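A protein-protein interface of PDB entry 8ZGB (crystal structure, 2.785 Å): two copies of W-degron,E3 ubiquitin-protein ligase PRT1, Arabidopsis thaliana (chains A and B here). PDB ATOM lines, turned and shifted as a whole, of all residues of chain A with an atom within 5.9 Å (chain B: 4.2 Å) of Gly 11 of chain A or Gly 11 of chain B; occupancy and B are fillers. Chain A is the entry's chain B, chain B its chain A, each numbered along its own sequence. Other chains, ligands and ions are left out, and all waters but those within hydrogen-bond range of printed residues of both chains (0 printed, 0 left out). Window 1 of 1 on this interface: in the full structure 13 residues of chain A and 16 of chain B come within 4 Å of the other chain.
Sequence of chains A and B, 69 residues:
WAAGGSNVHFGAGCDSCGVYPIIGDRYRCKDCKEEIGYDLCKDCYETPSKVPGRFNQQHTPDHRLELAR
The backbone carbonyl oxygen (O) of Phe 10 of chain A sits at hydrogen-bond distance from the side-chain hydroxyl (OH) of Tyr 20 of chain A, at 2.8 Å. The guanidinium group of Arg 26 of chain A lies within salt-bridge range of the side-chain carboxylate of Asp 39 of chain A (3.1 Å).
Ala 2 of chain A touches Gly 11 of chain B, and with the chains exchanged Gly 11 of chain A touches Ala 2 of chain B. Phe 10 of chain A touches Ala 3 of chain B, but with the chains exchanged Ala 3 of chain A does not touch Phe 10 of chain B (4.7 Å). Phe 10 of chain A touches Gly 11 of chain B, but with the chains exchanged Gly 11 of chain A does not touch Phe 10 of chain B (4.2 Å). Gly 11 of chain A touches its own counterpart, Gly 11 of chain B. 6 positions are printed for both chains.
Of the printed residues of chain B, Ala 2 of chain A touches Gly 11 (3.4 Å) and Ala 12 (3.9 Å). Gly 11 of chain A touches three residues of chain B. Gly 13 of chain A touches none of the printed residues of chain B. Of the printed residues of chain B, Asp 39 of chain A touches Ala 2. Of the printed residues of chain A, Phe 10 of chain B touches Phe 10 (3.3 Å) and Tyr 20 (3.8 Å). Gly 11 of chain B touches just these residues of chain A: Ala 2 (3.4 Å), Ala 3 (3.4 Å), Phe 10 (3.8 Å) and Gly 11 (3.5 Å). The nearest printed residue of chain B that does not touch Gly 11 of chain A is Phe 10 of chain B (4.2 Å). The nearest printed residue of chain A that does not touch Ala 12 of chain B is Ala 3 of chain A (4.2 Å).
Of the 11 printed residues of chain A, 8 touch a printed residue of chain B. Hydrophobic or aromatic side chains of chain A within 4 Å of the printed part of chain B: Ala 2, Phe 10 and Tyr 20. Hydrophobic or aromatic side chains of chain B within 4 Å of the printed part of chain A: Ala 3, Phe 10 and Ala 12. Among the printed residues, no Asp or Glu carboxylate lies within 4 Å of a Lys or Arg side-chain nitrogen of the other chain.
O of Gly 11 of chain A sits at hydrogen-bond distance from N of Ala 3 of chain B, at 3.3 Å. The backbone carbonyl oxygen of Gly 11 of chain B is in hydrogen-bond range of the backbone NH of Ala 3 of chain A (3.4 Å).
O of Gly 11 of chain B touches CA of Ala 2 of chain A, at 3.4 Å. CA of Ala 2 of chain A touches CA of Ala 12 of chain B, 3.9 Å away. Ala 3 of chain B touches Phe 10 of chain A (CB to O, 3.5 Å). Phe 10 of chain A touches Phe 10 of chain B (CB to O, 3.3 Å). Phe 10 of chain A touches Gly 11 of chain B (C to CA, 3.8 Å). Ala 2 of chain B touches Gly 11 of chain A. Gly 11 of chain A touches Gly 11 of chain B. Ala 12 of chain A touches Ala 3 of chain B. OH of Tyr 20 of chain A touches CB of Phe 10 of chain B, 3.8 Å away. Ala 2 of chain B touches Asp 39 of chain A.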
ATOM      1  N   TRP A   1      17.998 -10.760 -13.542  1.00  0.00           N
ATOM      2  CA  TRP A   1      18.774 -10.198 -14.642  1.00  0.00           C
ATOM      3  C   TRP A   1      18.397 -10.838 -15.968  1.00  0.00           C
ATOM      4  O   TRP A   1      18.457 -12.065 -16.130  1.00  0.00           O
ATOM      5  CB  TRP A   1      20.251 -10.392 -14.375  1.00  0.00           C
ATOM      6  CG  TRP A   1      20.610 -11.798 -14.054  1.00  0.00           C
ATOM      7  CD1 TRP A   1      20.632 -12.368 -12.823  1.00  0.00           C
ATOM      8  CD2 TRP A   1      20.970 -12.829 -14.983  1.00  0.00           C
ATOM      9  NE1 TRP A   1      21.000 -13.694 -12.922  1.00  0.00           N
ATOM     10  CE2 TRP A   1      21.222 -13.992 -14.240  1.00  0.00           C
ATOM     11  CE3 TRP A   1      21.118 -12.876 -16.369  1.00  0.00           C
ATOM     12  CZ2 TRP A   1      21.605 -15.185 -14.835  1.00  0.00           C
ATOM     13  CZ3 TRP A   1      21.498 -14.060 -16.958  1.00  0.00           C
ATOM     14  CH2 TRP A   1      21.733 -15.200 -16.194  1.00  0.00           C
ATOM     15  N   ALA A   2      17.967 -10.006 -16.911  1.00  0.00           N
ATOM     16  CA  ALA A   2      17.565 -10.487 -18.230  1.00  0.00           C
ATOM     17  C   ALA A   2      18.772 -10.780 -19.105  1.00  0.00           C
ATOM     18  O   ALA A   2      19.696  -9.972 -19.174  1.00  0.00           O
ATOM     19  CB  ALA A   2      16.665  -9.466 -18.932  1.00  0.00           C
ATOM     20  N   ALA A   3      18.776 -11.932 -19.767  1.00  0.00           N
ATOM     21  CA  ALA A   3      19.819 -12.202 -20.742  1.00  0.00           C
ATOM     22  C   ALA A   3      19.481 -11.361 -21.970  1.00  0.00           C
ATOM     23  O   ALA A   3      18.306 -11.097 -22.252  1.00  0.00           O
ATOM     24  CB  ALA A   3      19.876 -13.680 -21.068  1.00  0.00           C
ATOM     25  N   HIS A   9      16.241 -11.453 -27.253  1.00  0.00           N
ATOM     26  CA  HIS A   9      15.134 -11.805 -26.371  1.00  0.00           C
ATOM     27  C   HIS A   9      15.168 -13.313 -26.218  1.00  0.00           C
ATOM     28  O   HIS A   9      14.542 -14.030 -27.002  1.00  0.00           O
ATOM     29  CB  HIS A   9      13.812 -11.310 -26.942  1.00  0.00           C
ATOM     30  CG  HIS A   9      13.836  -9.869 -27.342  1.00  0.00           C
ATOM     31  ND1 HIS A   9      13.632  -8.841 -26.445  1.00  0.00           N
ATOM     32  CD2 HIS A   9      14.053  -9.281 -28.542  1.00  0.00           C
ATOM     33  CE1 HIS A   9      13.711  -7.683 -27.079  1.00  0.00           C
ATOM     34  NE2 HIS A   9      13.967  -7.922 -28.353  1.00  0.00           N
ATOM     35  N   PHE A  10      15.864 -13.793 -25.183  1.00  0.00           N
ATOM     36  CA  PHE A  10      15.991 -15.233 -25.009  1.00  0.00           C
ATOM     37  C   PHE A  10      14.724 -15.843 -24.417  1.00  0.00           C
ATOM     38  O   PHE A  10      14.621 -17.076 -24.344  1.00  0.00           O
ATOM     39  CB  PHE A  10      17.163 -15.610 -24.064  1.00  0.00           C
ATOM     40  CG  PHE A  10      18.515 -15.497 -24.705  1.00  0.00           C
ATOM     41  CD1 PHE A  10      18.962 -16.486 -25.579  1.00  0.00           C
ATOM     42  CD2 PHE A  10      19.346 -14.425 -24.433  1.00  0.00           C
ATOM     43  CE1 PHE A  10      20.203 -16.384 -26.209  1.00  0.00           C
ATOM     44  CE2 PHE A  10      20.596 -14.321 -25.045  1.00  0.00           C
ATOM     45  CZ  PHE A  10      21.023 -15.287 -25.946  1.00  0.00           C
ATOM     46  N   GLY A  11      13.773 -15.012 -23.987  1.00  0.00           N
ATOM     47  CA  GLY A  11      12.497 -15.458 -23.490  1.00  0.00           C
ATOM     48  C   GLY A  11      11.405 -15.523 -24.525  1.00  0.00           C
ATOM     49  O   GLY A  11      10.235 -15.664 -24.148  1.00  0.00           O
ATOM     50  N   ALA A  12      11.738 -15.418 -25.813  1.00  0.00           N
ATOM     51  CA  ALA A  12      10.698 -15.468 -26.825  1.00  0.00           C
ATOM     52  C   ALA A  12      11.278 -15.862 -28.170  1.00  0.00           C
ATOM     53  O   ALA A  12      12.457 -15.655 -28.446  1.00  0.00           O
ATOM     54  CB  ALA A  12       9.977 -14.118 -26.940  1.00  0.00           C
ATOM     55  N   GLY A  13      10.404 -16.404 -29.019  1.00  0.00           N
ATOM     56  CA  GLY A  13      10.763 -16.721 -30.387  1.00  0.00           C
ATOM     57  C   GLY A  13       9.659 -16.280 -31.325  1.00  0.00           C
ATOM     58  O   GLY A  13       8.509 -16.102 -30.919  1.00  0.00           O
ATOM     59  N   TYR A  20      14.903 -18.167 -33.064  1.00  0.00           N
ATOM     60  CA  TYR A  20      15.103 -18.102 -31.613  1.00  0.00           C
ATOM     61  C   TYR A  20      16.584 -18.053 -31.275  1.00  0.00           C
ATOM     62  O   TYR A  20      17.354 -18.891 -31.768  1.00  0.00           O
ATOM     63  CB  TYR A  20      14.459 -19.300 -30.916  1.00  0.00           C
ATOM     64  CG  TYR A  20      14.772 -19.353 -29.446  1.00  0.00           C
ATOM     65  CD1 TYR A  20      15.813 -20.150 -28.967  1.00  0.00           C
ATOM     66  CD2 TYR A  20      14.048 -18.601 -28.532  1.00  0.00           C
ATOM     67  CE1 TYR A  20      16.126 -20.184 -27.619  1.00  0.00           C
ATOM     68  CE2 TYR A  20      14.352 -18.642 -27.185  1.00  0.00           C
ATOM     69  CZ  TYR A  20      15.396 -19.428 -26.744  1.00  0.00           C
ATOM     70  OH  TYR A  20      15.696 -19.474 -25.411  1.00  0.00           O
ATOM     71  N   ARG A  26      11.454  -6.833 -31.155  1.00  0.00           N
ATOM     72  CA  ARG A  26      10.476  -7.875 -30.877  1.00  0.00           C
ATOM     73  C   ARG A  26       9.115  -7.215 -30.705  1.00  0.00           C
ATOM     74  O   ARG A  26       8.986  -6.199 -30.004  1.00  0.00           O
ATOM     75  CB  ARG A  26      10.830  -8.668 -29.622  1.00  0.00           C
ATOM     76  CG  ARG A  26       9.639  -9.377 -28.953  1.00  0.00           C
ATOM     77  CD  ARG A  26      10.096 -10.138 -27.698  1.00  0.00           C
ATOM     78  NE  ARG A  26       8.989 -10.797 -27.001  1.00  0.00           N
ATOM     79  CZ  ARG A  26       8.959 -11.049 -25.689  1.00  0.00           C
ATOM     80  NH1 ARG A  26       9.982 -10.691 -24.913  1.00  0.00           N
ATOM     81  NH2 ARG A  26       7.908 -11.668 -25.157  1.00  0.00           N
ATOM     82  N   ASP A  39       4.617 -13.781 -30.401  1.00  0.00           N
ATOM     83  CA  ASP A  39       5.738 -12.882 -30.617  1.00  0.00           C
ATOM     84  C   ASP A  39       6.137 -12.930 -32.083  1.00  0.00           C
ATOM     85  O   ASP A  39       5.915 -13.927 -32.784  1.00  0.00           O
ATOM     86  CB  ASP A  39       6.925 -13.264 -29.714  1.00  0.00           C
ATOM     87  CG  ASP A  39       6.509 -13.440 -28.262  1.00  0.00           C
ATOM     88  OD1 ASP A  39       6.442 -14.599 -27.791  1.00  0.00           O
ATOM     89  OD2 ASP A  39       6.187 -12.414 -27.614  1.00  0.00           O
ATOM     90  N   ALA B   2       6.562 -17.909 -26.079  1.00  0.00           N
ATOM     91  CA  ALA B   2       7.412 -17.890 -24.900  1.00  0.00           C
ATOM     92  C   ALA B   2       8.352 -19.094 -24.939  1.00  0.00           C
ATOM     93  O   ALA B   2       7.931 -20.238 -25.128  1.00  0.00           O
ATOM     94  CB  ALA B   2       6.548 -17.932 -23.640  1.00  0.00           C
ATOM     95  N   ALA B   3       9.628 -18.836 -24.736  1.00  0.00           N
ATOM     96  CA  ALA B   3      10.628 -19.891 -24.711  1.00  0.00           C
ATOM     97  C   ALA B   3      10.627 -20.598 -23.362  1.00  0.00           C
ATOM     98  O   ALA B   3      10.649 -19.953 -22.301  1.00  0.00           O
ATOM     99  CB  ALA B   3      12.014 -19.308 -24.983  1.00  0.00           C
ATOM    100  N   HIS B   9      11.632 -19.712 -17.634  1.00  0.00           N
ATOM    101  CA  HIS B   9      11.828 -18.371 -18.183  1.00  0.00           C
ATOM    102  C   HIS B   9      13.286 -18.268 -18.624  1.00  0.00           C
ATOM    103  O   HIS B   9      14.165 -17.918 -17.836  1.00  0.00           O
ATOM    104  CB  HIS B   9      11.448 -17.301 -17.167  1.00  0.00           C
ATOM    105  CG  HIS B   9      10.092 -17.499 -16.570  1.00  0.00           C
ATOM    106  ND1 HIS B   9       8.961 -16.911 -17.096  1.00  0.00           N
ATOM    107  CD2 HIS B   9       9.680 -18.228 -15.504  1.00  0.00           C
ATOM    108  CE1 HIS B   9       7.911 -17.265 -16.374  1.00  0.00           C
ATOM    109  NE2 HIS B   9       8.318 -18.067 -15.405  1.00  0.00           N
ATOM    110  N   PHE B  10      13.535 -18.594 -19.889  1.00  0.00           N
ATOM    111  CA  PHE B  10      14.890 -18.565 -20.421  1.00  0.00           C
ATOM    112  C   PHE B  10      15.382 -17.159 -20.692  1.00  0.00           C
ATOM    113  O   PHE B  10      16.538 -16.999 -21.091  1.00  0.00           O
ATOM    114  CB  PHE B  10      14.982 -19.372 -21.722  1.00  0.00           C
ATOM    115  CG  PHE B  10      15.105 -20.862 -21.505  1.00  0.00           C
ATOM    116  CD1 PHE B  10      14.041 -21.712 -21.778  1.00  0.00           C
ATOM    117  CD2 PHE B  10      16.317 -21.415 -21.056  1.00  0.00           C
ATOM    118  CE1 PHE B  10      14.155 -23.069 -21.582  1.00  0.00           C
ATOM    119  CE2 PHE B  10      16.446 -22.793 -20.871  1.00  0.00           C
ATOM    120  CZ  PHE B  10      15.365 -23.615 -21.136  1.00  0.00           C
ATOM    121  N   GLY B  11      14.545 -16.149 -20.493  1.00  0.00           N
ATOM    122  CA  GLY B  11      14.915 -14.774 -20.734  1.00  0.00           C
ATOM    123  C   GLY B  11      15.363 -13.996 -19.525  1.00  0.00           C
ATOM    124  O   GLY B  11      15.515 -12.771 -19.615  1.00  0.00           O
ATOM    125  N   ALA B  12      15.575 -14.655 -18.396  1.00  0.00           N
ATOM    126  CA  ALA B  12      16.045 -13.952 -17.213  1.00  0.00           C
ATOM    127  C   ALA B  12      16.608 -14.948 -16.206  1.00  0.00           C
ATOM    128  O   ALA B  12      16.273 -16.136 -16.213  1.00  0.00           O
ATOM    129  CB  ALA B  12      14.917 -13.121 -16.580  1.00  0.00           C
